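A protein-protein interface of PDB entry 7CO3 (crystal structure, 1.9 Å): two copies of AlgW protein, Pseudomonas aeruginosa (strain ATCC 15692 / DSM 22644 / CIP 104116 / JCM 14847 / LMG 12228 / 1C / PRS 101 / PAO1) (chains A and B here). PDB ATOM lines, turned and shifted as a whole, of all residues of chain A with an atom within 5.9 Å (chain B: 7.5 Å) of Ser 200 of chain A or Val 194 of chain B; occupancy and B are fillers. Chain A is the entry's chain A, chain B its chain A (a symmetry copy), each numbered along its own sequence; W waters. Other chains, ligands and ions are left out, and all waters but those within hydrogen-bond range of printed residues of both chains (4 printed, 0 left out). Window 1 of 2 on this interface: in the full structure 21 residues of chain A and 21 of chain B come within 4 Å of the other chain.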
ATOM      1  N   THR A 177      -2.509 -12.592   9.904  1.00  0.00           N
ATOM      2  CA  THR A 177      -2.781 -12.875  11.309  1.00  0.00           C
ATOM      3  C   THR A 177      -1.638 -12.393  12.191  1.00  0.00           C
ATOM      4  O   THR A 177      -0.466 -12.650  11.916  1.00  0.00           O
ATOM      5  CB  THR A 177      -3.011 -14.376  11.489  1.00  0.00           C
ATOM      6  OG1 THR A 177      -4.206 -14.723  10.798  1.00  0.00           O
ATOM      7  CG2 THR A 177      -3.135 -14.789  12.971  1.00  0.00           C
ATOM      8  N   GLY A 178      -1.982 -11.677  13.258  1.00  0.00           N
ATOM      9  CA  GLY A 178      -0.986 -11.051  14.086  1.00  0.00           C
ATOM     10  C   GLY A 178      -0.811  -9.569  13.836  1.00  0.00           C
ATOM     11  O   GLY A 178      -0.227  -8.891  14.672  1.00  0.00           O
ATOM     12  N   ILE A 198      -5.674  -7.655  17.559  1.00  0.00           N
ATOM     13  CA  ILE A 198      -4.967  -8.160  16.375  1.00  0.00           C
ATOM     14  C   ILE A 198      -5.943  -8.918  15.490  1.00  0.00           C
ATOM     15  O   ILE A 198      -7.021  -9.334  15.925  1.00  0.00           O
ATOM     16  CB  ILE A 198      -3.773  -9.100  16.687  1.00  0.00           C
ATOM     17  CG1 ILE A 198      -4.250 -10.330  17.497  1.00  0.00           C
ATOM     18  CG2 ILE A 198      -2.599  -8.374  17.382  1.00  0.00           C
ATOM     19  CD1 ILE A 198      -3.246 -11.473  17.476  1.00  0.00           C
ATOM     20  N   ILE A 199      -5.539  -9.100  14.231  1.00  0.00           N
ATOM     21  CA  ILE A 199      -6.161 -10.111  13.373  1.00  0.00           C
ATOM     22  C   ILE A 199      -5.898 -11.466  14.005  1.00  0.00           C
ATOM     23  O   ILE A 199      -4.742 -11.887  14.107  1.00  0.00           O
ATOM     24  CB  ILE A 199      -5.593 -10.057  11.941  1.00  0.00           C
ATOM     25  CG1 ILE A 199      -5.721  -8.666  11.333  1.00  0.00           C
ATOM     26  CG2 ILE A 199      -6.232 -11.152  11.036  1.00  0.00           C
ATOM     27  CD1 ILE A 199      -7.143  -8.098  11.364  1.00  0.00           C
ATOM     28  N   SER A 200      -6.971 -12.153  14.419  1.00  0.00           N
ATOM     29  CA  SER A 200      -6.873 -13.447  15.082  1.00  0.00           C
ATOM     30  C   SER A 200      -6.840 -14.603  14.093  1.00  0.00           C
ATOM     31  O   SER A 200      -6.356 -15.692  14.431  1.00  0.00           O
ATOM     32  CB  SER A 200      -8.037 -13.628  16.053  1.00  0.00           C
ATOM     33  OG  SER A 200      -7.870 -12.747  17.142  1.00  0.00           O
ATOM     34  N   ALA A 201      -7.402 -14.392  12.909  1.00  0.00           N
ATOM     35  CA  ALA A 201      -7.533 -15.388  11.841  1.00  0.00           C
ATOM     36  C   ALA A 201      -8.275 -14.714  10.695  1.00  0.00           C
ATOM     37  O   ALA A 201      -8.903 -13.654  10.859  1.00  0.00           O
ATOM     38  CB  ALA A 201      -8.262 -16.659  12.290  1.00  0.00           C
ATOM     39  N   THR A 202      -8.172 -15.322   9.520  1.00  0.00           N
ATOM     40  CA  THR A 202      -8.888 -14.838   8.353  1.00  0.00           C
ATOM     41  C   THR A 202      -9.589 -16.009   7.664  1.00  0.00           C
ATOM     42  O   THR A 202      -9.315 -17.179   7.937  1.00  0.00           O
ATOM     43  CB  THR A 202      -7.956 -14.100   7.361  1.00  0.00           C
ATOM     44  OG1 THR A 202      -7.094 -15.069   6.745  1.00  0.00           O
ATOM     45  CG2 THR A 202      -7.085 -13.058   8.062  1.00  0.00           C
ATOM     46  N   ARG A 204     -12.821 -16.933   7.790  1.00  0.00           N
ATOM     47  CA  ARG A 204     -13.755 -17.712   8.608  1.00  0.00           C
ATOM     48  C   ARG A 204     -15.076 -17.852   7.863  1.00  0.00           C
ATOM     49  O   ARG A 204     -15.923 -16.947   7.826  1.00  0.00           O
ATOM     50  CB  ARG A 204     -13.963 -17.063   9.972  1.00  0.00           C
ATOM     51  CG  ARG A 204     -12.746 -17.205  10.867  1.00  0.00           C
ATOM     52  CD  ARG A 204     -12.633 -18.592  11.468  1.00  0.00           C
ATOM     53  NE  ARG A 204     -11.850 -18.540  12.687  1.00  0.00           N
ATOM     54  CZ  ARG A 204     -10.680 -19.139  12.887  1.00  0.00           C
ATOM     55  NH1 ARG A 204     -10.107 -19.851  11.929  1.00  0.00           N
ATOM     56  NH2 ARG A 204     -10.063 -19.002  14.062  1.00  0.00           N
ATOM     57  N   ILE A 216     -12.939 -12.028   8.610  1.00  0.00           N
ATOM     58  CA  ILE A 216     -11.802 -11.726   9.458  1.00  0.00           C
ATOM     59  C   ILE A 216     -12.240 -11.894  10.907  1.00  0.00           C
ATOM     60  O   ILE A 216     -13.350 -11.470  11.280  1.00  0.00           O
ATOM     61  CB  ILE A 216     -11.311 -10.297   9.191  1.00  0.00           C
ATOM     62  CG1 ILE A 216     -10.934 -10.140   7.708  1.00  0.00           C
ATOM     63  CG2 ILE A 216     -10.106 -10.004  10.054  1.00  0.00           C
ATOM     64  CD1 ILE A 216     -10.815  -8.643   7.250  1.00  0.00           C
ATOM     65  N   GLN A 217     -11.394 -12.532  11.715  1.00  0.00           N
ATOM     66  CA  GLN A 217     -11.597 -12.675  13.156  1.00  0.00           C
ATOM     67  C   GLN A 217     -10.657 -11.713  13.892  1.00  0.00           C
ATOM     68  O   GLN A 217      -9.507 -11.522  13.488  1.00  0.00           O
ATOM     69  CB  GLN A 217     -11.375 -14.132  13.590  1.00  0.00           C
ATOM     70  CG  GLN A 217     -11.874 -14.463  14.995  1.00  0.00           C
ATOM     71  CD  GLN A 217     -11.585 -15.891  15.414  1.00  0.00           C
ATOM     72  OE1 GLN A 217     -11.835 -16.845  14.671  1.00  0.00           O
ATOM     73  NE2 GLN A 217     -11.041 -16.045  16.630  1.00  0.00           N
ATOM     74  N   THR A 218     -11.132 -11.077  14.974  1.00  0.00           N
ATOM     75  CA  THR A 218     -10.270 -10.134  15.692  1.00  0.00           C
ATOM     76  C   THR A 218     -10.560 -10.203  17.179  1.00  0.00           C
ATOM     77  O   THR A 218     -11.691 -10.462  17.578  1.00  0.00           O
ATOM     78  CB  THR A 218     -10.464  -8.673  15.209  1.00  0.00           C
ATOM     79  OG1 THR A 218      -9.612  -7.803  15.947  1.00  0.00           O
ATOM     80  CG2 THR A 218     -11.920  -8.213  15.409  1.00  0.00           C
ATOM     81  N   ASP A 219      -9.535  -9.958  18.011  1.00  0.00           N
ATOM     82  CA  ASP A 219      -9.824  -9.851  19.439  1.00  0.00           C
ATOM     83  C   ASP A 219     -10.009  -8.403  19.898  1.00  0.00           C
ATOM     84  O   ASP A 219     -10.205  -8.184  21.084  1.00  0.00           O
ATOM     85  CB  ASP A 219      -8.779 -10.590  20.285  1.00  0.00           C
ATOM     86  CG  ASP A 219      -7.372 -10.007  20.158  1.00  0.00           C
ATOM     87  OD1 ASP A 219      -7.147  -9.121  19.299  1.00  0.00           O
ATOM     88  OD2 ASP A 219      -6.480 -10.452  20.930  1.00  0.00           O
ATOM     89  N   GLY A 254     -13.562 -11.364  23.187  1.00  0.00           N
ATOM     90  CA  GLY A 254     -12.388 -11.362  22.331  1.00  0.00           C
ATOM     91  C   GLY A 254     -12.495 -12.195  21.059  1.00  0.00           C
ATOM     92  O   GLY A 254     -11.469 -12.441  20.425  1.00  0.00           O
ATOM     93  N   TYR B  55       2.593  -8.596  14.833  1.00  0.00           N
ATOM     94  CA  TYR B  55       3.056  -9.850  15.396  1.00  0.00           C
ATOM     95  C   TYR B  55       2.960 -10.983  14.384  1.00  0.00           C
ATOM     96  O   TYR B  55       3.070 -12.148  14.752  1.00  0.00           O
ATOM     97  CB  TYR B  55       2.282 -10.152  16.680  1.00  0.00           C
ATOM     98  CG  TYR B  55       2.399  -8.972  17.646  1.00  0.00           C
ATOM     99  CD1 TYR B  55       3.573  -8.782  18.395  1.00  0.00           C
ATOM    100  CD2 TYR B  55       1.378  -8.019  17.773  1.00  0.00           C
ATOM    101  CE1 TYR B  55       3.722  -7.727  19.232  1.00  0.00           C
ATOM    102  CE2 TYR B  55       1.524  -6.936  18.639  1.00  0.00           C
ATOM    103  CZ  TYR B  55       2.699  -6.812  19.367  1.00  0.00           C
ATOM    104  OH  TYR B  55       2.896  -5.763  20.209  1.00  0.00           O
ATOM    105  N   ALA B  58       5.899 -13.504  14.454  1.00  0.00           N
ATOM    106  CA  ALA B  58       5.768 -14.391  15.611  1.00  0.00           C
ATOM    107  C   ALA B  58       4.689 -15.447  15.380  1.00  0.00           C
ATOM    108  O   ALA B  58       4.890 -16.626  15.691  1.00  0.00           O
ATOM    109  CB  ALA B  58       5.499 -13.574  16.873  1.00  0.00           C
ATOM    110  N   VAL B  59       3.543 -15.060  14.798  1.00  0.00           N
ATOM    111  CA  VAL B  59       2.496 -16.053  14.530  1.00  0.00           C
ATOM    112  C   VAL B  59       2.984 -17.072  13.502  1.00  0.00           C
ATOM    113  O   VAL B  59       2.819 -18.282  13.673  1.00  0.00           O
ATOM    114  CB  VAL B  59       1.193 -15.379  14.044  1.00  0.00           C
ATOM    115  CG1 VAL B  59       0.248 -16.439  13.351  1.00  0.00           C
ATOM    116  CG2 VAL B  59       0.473 -14.586  15.164  1.00  0.00           C
ATOM    117  N   SER B  60       3.571 -16.587  12.409  1.00  0.00           N
ATOM    118  CA  SER B  60       4.106 -17.483  11.391  1.00  0.00           C
ATOM    119  C   SER B  60       5.051 -18.508  12.007  1.00  0.00           C
ATOM    120  O   SER B  60       5.064 -19.680  11.611  1.00  0.00           O
ATOM    121  CB  SER B  60       4.798 -16.672  10.305  1.00  0.00           C
ATOM    122  OG  SER B  60       3.835 -16.187   9.384  1.00  0.00           O
ATOM    123  N   ALA B  63       2.490 -20.684  15.168  1.00  0.00           N
ATOM    124  CA  ALA B  63       1.211 -21.318  14.863  1.00  0.00           C
ATOM    125  C   ALA B  63       1.338 -22.718  14.248  1.00  0.00           C
ATOM    126  O   ALA B  63       0.521 -23.587  14.603  1.00  0.00           O
ATOM    127  CB  ALA B  63       0.396 -20.393  13.962  1.00  0.00           C
ATOM    128  N   CYS B 181       2.406 -10.742  24.950  1.00  0.00           N
ATOM    129  CA  CYS B 181       2.353 -12.174  24.637  1.00  0.00           C
ATOM    130  C   CYS B 181       1.152 -12.488  23.755  1.00  0.00           C
ATOM    131  O   CYS B 181       0.195 -11.707  23.637  1.00  0.00           O
ATOM    132  CB  CYS B 181       2.291 -13.054  25.903  1.00  0.00           C
ATOM    133  SG  CYS B 181       0.926 -12.543  26.988  1.00  0.00           S
ATOM    134  N   LEU B 182       1.205 -13.676  23.162  1.00  0.00           N
ATOM    135  CA  LEU B 182       0.196 -14.182  22.238  1.00  0.00           C
ATOM    136  C   LEU B 182      -0.309 -15.538  22.734  1.00  0.00           C
ATOM    137  O   LEU B 182       0.495 -16.400  23.093  1.00  0.00           O
ATOM    138  CB  LEU B 182       0.815 -14.327  20.844  1.00  0.00           C
ATOM    139  CG  LEU B 182       1.006 -13.131  19.918  1.00  0.00           C
ATOM    140  CD1 LEU B 182       1.561 -11.928  20.588  1.00  0.00           C
ATOM    141  CD2 LEU B 182       1.950 -13.534  18.791  1.00  0.00           C
ATOM    142  N   ALA B 183      -1.641 -15.729  22.769  1.00  0.00           N
ATOM    143  CA  ALA B 183      -2.261 -17.012  23.058  1.00  0.00           C
ATOM    144  C   ALA B 183      -2.689 -17.647  21.730  1.00  0.00           C
ATOM    145  O   ALA B 183      -3.207 -16.956  20.848  1.00  0.00           O
ATOM    146  CB  ALA B 183      -3.475 -16.850  23.982  1.00  0.00           C
ATOM    147  N   ILE B 184      -2.485 -18.955  21.594  1.00  0.00           N
ATOM    148  CA  ILE B 184      -2.788 -19.698  20.360  1.00  0.00           C
ATOM    149  C   ILE B 184      -3.580 -20.927  20.743  1.00  0.00           C
ATOM    150  O   ILE B 184      -3.111 -21.744  21.528  1.00  0.00           O
ATOM    151  CB  ILE B 184      -1.531 -20.090  19.553  1.00  0.00           C
ATOM    152  CG1 ILE B 184      -0.643 -18.880  19.319  1.00  0.00           C
ATOM    153  CG2 ILE B 184      -1.947 -20.642  18.186  1.00  0.00           C
ATOM    154  CD1 ILE B 184       0.611 -19.161  18.533  1.00  0.00           C
ATOM    155  N   GLY B 185      -4.794 -21.034  20.224  1.00  0.00           N
ATOM    156  CA  GLY B 185      -5.653 -22.130  20.616  1.00  0.00           C
ATOM    157  C   GLY B 185      -6.880 -22.188  19.740  1.00  0.00           C
ATOM    158  O   GLY B 185      -6.944 -21.556  18.685  1.00  0.00           O
ATOM    159  N   ASN B 186      -7.859 -22.973  20.190  1.00  0.00           N
ATOM    160  CA  ASN B 186      -9.090 -23.220  19.435  1.00  0.00           C
ATOM    161  C   ASN B 186     -10.314 -22.802  20.260  1.00  0.00           C
ATOM    162  O   ASN B 186     -11.142 -23.654  20.625  1.00  0.00           O
ATOM    163  CB  ASN B 186      -9.196 -24.697  19.022  1.00  0.00           C
ATOM    164  CG  ASN B 186     -10.297 -24.940  17.931  1.00  0.00           C
ATOM    165  OD1 ASN B 186     -10.852 -24.002  17.342  1.00  0.00           O
ATOM    166  ND2 ASN B 186     -10.627 -26.224  17.716  1.00  0.00           N
ATOM    167  N   PRO B 187     -10.474 -21.509  20.569  1.00  0.00           N
ATOM    168  CA  PRO B 187     -11.585 -21.105  21.451  1.00  0.00           C
ATOM    169  C   PRO B 187     -12.932 -21.424  20.825  1.00  0.00           C
ATOM    170  O   PRO B 187     -13.178 -21.151  19.653  1.00  0.00           O
ATOM    171  CB  PRO B 187     -11.390 -19.595  21.603  1.00  0.00           C
ATOM    172  CG  PRO B 187     -10.620 -19.196  20.421  1.00  0.00           C
ATOM    173  CD  PRO B 187      -9.695 -20.346  20.150  1.00  0.00           C
ATOM    174  N   GLY B 191     -11.781 -22.623  15.297  1.00  0.00           N
ATOM    175  CA  GLY B 191     -10.551 -22.676  14.532  1.00  0.00           C
ATOM    176  C   GLY B 191      -9.384 -22.138  15.331  1.00  0.00           C
ATOM    177  O   GLY B 191      -9.541 -21.497  16.367  1.00  0.00           O
ATOM    178  N   GLN B 192      -8.197 -22.494  14.863  1.00  0.00           N
ATOM    179  CA  GLN B 192      -7.002 -21.931  15.458  1.00  0.00           C
ATOM    180  C   GLN B 192      -7.113 -20.416  15.480  1.00  0.00           C
ATOM    181  O   GLN B 192      -7.428 -19.791  14.465  1.00  0.00           O
ATOM    182  CB  GLN B 192      -5.760 -22.313  14.679  1.00  0.00           C
ATOM    183  CG  GLN B 192      -4.554 -22.028  15.538  1.00  0.00           C
ATOM    184  CD  GLN B 192      -3.253 -22.199  14.797  1.00  0.00           C
ATOM    185  OE1 GLN B 192      -2.964 -21.481  13.833  1.00  0.00           O
ATOM    186  NE2 GLN B 192      -2.445 -23.154  15.264  1.00  0.00           N
ATOM    187  N   THR B 193      -6.803 -19.833  16.632  1.00  0.00           N
ATOM    188  CA  THR B 193      -7.085 -18.431  16.901  1.00  0.00           C
ATOM    189  C   THR B 193      -5.903 -17.814  17.635  1.00  0.00           C
ATOM    190  O   THR B 193      -5.383 -18.404  18.577  1.00  0.00           O
ATOM    191  CB  THR B 193      -8.370 -18.294  17.753  1.00  0.00           C
ATOM    192  OG1 THR B 193      -9.531 -18.632  16.978  1.00  0.00           O
ATOM    193  CG2 THR B 193      -8.507 -16.837  18.341  1.00  0.00           C
ATOM    194  N   VAL B 194      -5.464 -16.640  17.214  1.00  0.00           N
ATOM    195  CA  VAL B 194      -4.383 -15.947  17.910  1.00  0.00           C
ATOM    196  C   VAL B 194      -4.973 -14.742  18.620  1.00  0.00           C
ATOM    197  O   VAL B 194      -5.619 -13.922  17.989  1.00  0.00           O
ATOM    198  CB  VAL B 194      -3.237 -15.515  16.970  1.00  0.00           C
ATOM    199  CG1 VAL B 194      -2.072 -14.899  17.819  1.00  0.00           C
ATOM    200  CG2 VAL B 194      -2.720 -16.702  16.188  1.00  0.00           C
ATOM    201  N   THR B 195      -4.714 -14.611  19.916  1.00  0.00           N
ATOM    202  CA  THR B 195      -5.074 -13.398  20.642  1.00  0.00           C
ATOM    203  C   THR B 195      -3.834 -12.774  21.261  1.00  0.00           C
ATOM    204  O   THR B 195      -2.855 -13.450  21.509  1.00  0.00           O
ATOM    205  CB  THR B 195      -6.121 -13.674  21.717  1.00  0.00           C
ATOM    206  OG1 THR B 195      -5.653 -14.747  22.545  1.00  0.00           O
ATOM    207  CG2 THR B 195      -7.425 -14.086  21.094  1.00  0.00           C
ATOM    208  N   MET B 196      -3.913 -11.479  21.562  1.00  0.00           N
ATOM    209  CA  MET B 196      -2.765 -10.711  22.003  1.00  0.00           C
ATOM    210  C   MET B 196      -3.079  -9.985  23.303  1.00  0.00           C
ATOM    211  O   MET B 196      -4.184  -9.454  23.475  1.00  0.00           O
ATOM    212  CB  MET B 196      -2.375  -9.697  20.932  1.00  0.00           C
ATOM    213  CG  MET B 196      -1.093  -8.981  21.223  1.00  0.00           C
ATOM    214  SD  MET B 196      -1.370  -7.434  22.137  1.00  0.00           S
ATOM    215  CE  MET B 196      -2.328  -6.489  20.922  1.00  0.00           C
ATOM    216  N   ALA B 220      -4.392 -11.602  27.369  1.00  0.00           N
ATOM    217  CA  ALA B 220      -4.751 -12.124  26.044  1.00  0.00           C
ATOM    218  C   ALA B 220      -6.008 -12.982  26.167  1.00  0.00           C
ATOM    219  O   ALA B 220      -6.093 -13.837  27.045  1.00  0.00           O
ATOM    220  CB  ALA B 220      -3.604 -12.923  25.447  1.00  0.00           C
ATOM    221  N   ALA B 221      -7.008 -12.712  25.317  1.00  0.00           N
ATOM    222  CA  ALA B 221      -8.325 -13.336  25.488  1.00  0.00           C
ATOM    223  C   ALA B 221      -8.148 -14.843  25.415  1.00  0.00           C
ATOM    224  O   ALA B 221      -7.544 -15.369  24.473  1.00  0.00           O
ATOM    225  CB  ALA B 221      -9.334 -12.857  24.429  1.00  0.00           C
ATOM    226  N   ASN B 226      -9.171 -23.003  24.573  1.00  0.00           N
ATOM    227  CA  ASN B 226      -7.747 -22.617  24.574  1.00  0.00           C
ATOM    228  C   ASN B 226      -6.865 -23.569  25.397  1.00  0.00           C
ATOM    229  O   ASN B 226      -5.629 -23.519  25.279  1.00  0.00           O
ATOM    230  CB  ASN B 226      -7.565 -21.199  25.129  1.00  0.00           C
ATOM    231  CG  ASN B 226      -7.733 -20.110  24.062  1.00  0.00           C
ATOM    232  OD1 ASN B 226      -8.778 -19.488  23.985  1.00  0.00           O
ATOM    233  ND2 ASN B 226      -6.712 -19.881  23.254  1.00  0.00           N
ATOM    234  N   VAL B 232       2.836 -17.497  23.918  1.00  0.00           N
ATOM    235  CA  VAL B 232       4.080 -17.231  23.211  1.00  0.00           C
ATOM    236  C   VAL B 232       4.508 -15.787  23.457  1.00  0.00           C
ATOM    237  O   VAL B 232       3.665 -14.921  23.677  1.00  0.00           O
ATOM    238  CB  VAL B 232       3.793 -17.586  21.734  1.00  0.00           C
ATOM    239  CG1 VAL B 232       4.009 -16.459  20.773  1.00  0.00           C
ATOM    240  CG2 VAL B 232       4.403 -18.919  21.354  1.00  0.00           C
HETATM  241  O   HOH W   1      -7.090 -10.352  23.730  1.00  0.00           O
HETATM  242  O   HOH W   2       1.301 -14.269  10.293  1.00  0.00           O
HETATM  243  O   HOH W   3      -5.464 -18.035  13.212  1.00  0.00           O
HETATM  244  O   HOH W   4      -5.455  -7.891  21.584  1.00  0.00           O
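The backbone carbonyl oxygen of Val 194 of chain B sits at hydrogen-bond distance from the side-chain hydroxyl of Ser 200 of chain A, 2.7 Å away.
The guanidinium group (NH2) of Arg 204 of chain A is in hydrogen-bond range of the backbone carbonyl oxygen (O) of Gly 191 of chain B, at 3.4 Å.
OG1 of Thr 193 of chain B is in hydrogen-bond range of NH2 of Arg 204 of chain A, at 3.0 Å.
O of Gly 178 of chain A lies within hydrogen-bond range of N of Tyr 55 of chain B, 2.8 Å away.
OD2 of Asp 219 of chain A sits at hydrogen-bond distance from N of Met 196 of chain B (2.8 Å).
NH2 of Arg 204 of chain A lies within hydrogen-bond range of O of Gln 192 of chain B (2.8 Å).
The side-chain amide nitrogen (NE2) of Gln 217 of chain A is in hydrogen-bond range of the side-chain hydroxyl (OG1) of Thr 193 of chain B.
The backbone NH (N) of Ser 200 of chain A is in hydrogen-bond range of the backbone carbonyl oxygen (O) of Gln 217 of chain A (2.8 Å).
The backbone carbonyl oxygen (O) of Ala 201 of chain A lies within hydrogen-bond range of the backbone NH (N) of Gln 217 of chain A (2.9 Å).
The backbone NH (N) of Gly 178 of chain A lies within hydrogen-bond range of the backbone carbonyl oxygen (O) of Ile 199 of chain A, 2.9 Å away.
The backbone NH of Ile 198 of chain A lies within hydrogen-bond range of the side-chain carboxylate of Asp 219 of chain A.
The backbone carbonyl oxygen (O) of Gly 191 of chain B lies within hydrogen-bond range of the side-chain hydroxyl (OG1) of Thr 193 of chain B, 2.9 Å away.
The backbone carbonyl oxygen (O) of Ala 63 of chain B sits at hydrogen-bond distance from the side-chain amide nitrogen (NE2) of Gln 192 of chain B (3.1 Å).
Val 59 of chain B touches Thr 177 of chain A.
CG2 of Thr 177 of chain A touches CG2 of Val 194 of chain B, 3.8 Å away.
CA of Gly 178 of chain A touches CG2 of Val 59 of chain B (3.97 Å).
O of Val 194 of chain B touches CD1 of Ile 198 of chain A, 3.4 Å away.
Ile 198 of chain A touches Met 196 of chain B (CG2 to CB, 3.8 Å).
Ser 200 of chain A touches Thr 193 of chain B (O to CA, 3.8 Å).
Ala 201 of chain A touches Gln 192 of chain B.
OD2 of Asp 219 of chain A touches CA of Thr 195 of chain B, 3.3 Å away.
CA of Gly 254 of chain A touches CB of Ala 221 of chain B, at 3.995 Å.
Of chain B, only Thr 193 and Val 194 come within 4 Å of Ser 200 of chain A.
Of chain A, only Thr 177 (3.8 Å), Ile 198 (3.4 Å) and Ser 200 (2.7 Å) come within 4 Å of Val 194 of chain B.
Of the printed residues of chain A, Met 196 of chain B touches Ile 198 and Asp 219.
Of the printed residues of chain A, Tyr 55 of chain B touches Gly 178 (2.8 Å).
Of the printed residues of chain B, Gln 217 of chain A touches Thr 193 (3.0 Å).
Of the printed residues of chain B, Asp 219 of chain A touches Thr 195 and Met 196.
Gly 185 of chain B touches none of the printed residues of chain A.
The nearest residue of chain A that does not touch Val 194 of chain B is Ile 199 of chain A (4.5 Å).
The nearest printed residue of chain B that does not touch Asp 219 of chain A is Val 194 of chain B (4.6 Å).
Hydrophobic or aromatic side chains of chain B that line the printed part of chain A: Tyr 55, Val 59, Val 194, Met 196 and Ala 221.
Of the 13 printed residues of chain A, 9 touch a printed residue of chain B.
Hydrophobic or aromatic side chains of chain A within 4 Å of the printed part of chain B: Ile 198 and Ala 201.
Along chain A the printed residues that touch a printed residue of chain B span positions 177 to 254.
Among the printed residues, 16 pairs touch across the chains.
No position is printed for both chains.
Of the 16 pairs that touch across the chains among the printed residues, none has its exchanged pair printed and touching as well.
Water W4 lies within hydrogen-bond range of O of Met 196 of chain B and OD2 of Asp 219 of chain A.
Water W3 bridges the backbone carbonyl oxygen of Ser 200 of chain A (2.8 Å) and the backbone carbonyl oxygen of Gln 192 of chain B (2.9 Å).
Water W1 lies within hydrogen-bond range of the backbone NH of Ala 221 of chain B, the side-chain carboxylate of Asp 219 of chain A and the backbone carbonyl oxygen of Met 196 of chain B.
Water W2 lies within hydrogen-bond range of O of Thr 177 of chain A (2.9 Å) and OG of Ser 60 of chain B (3.3 Å).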
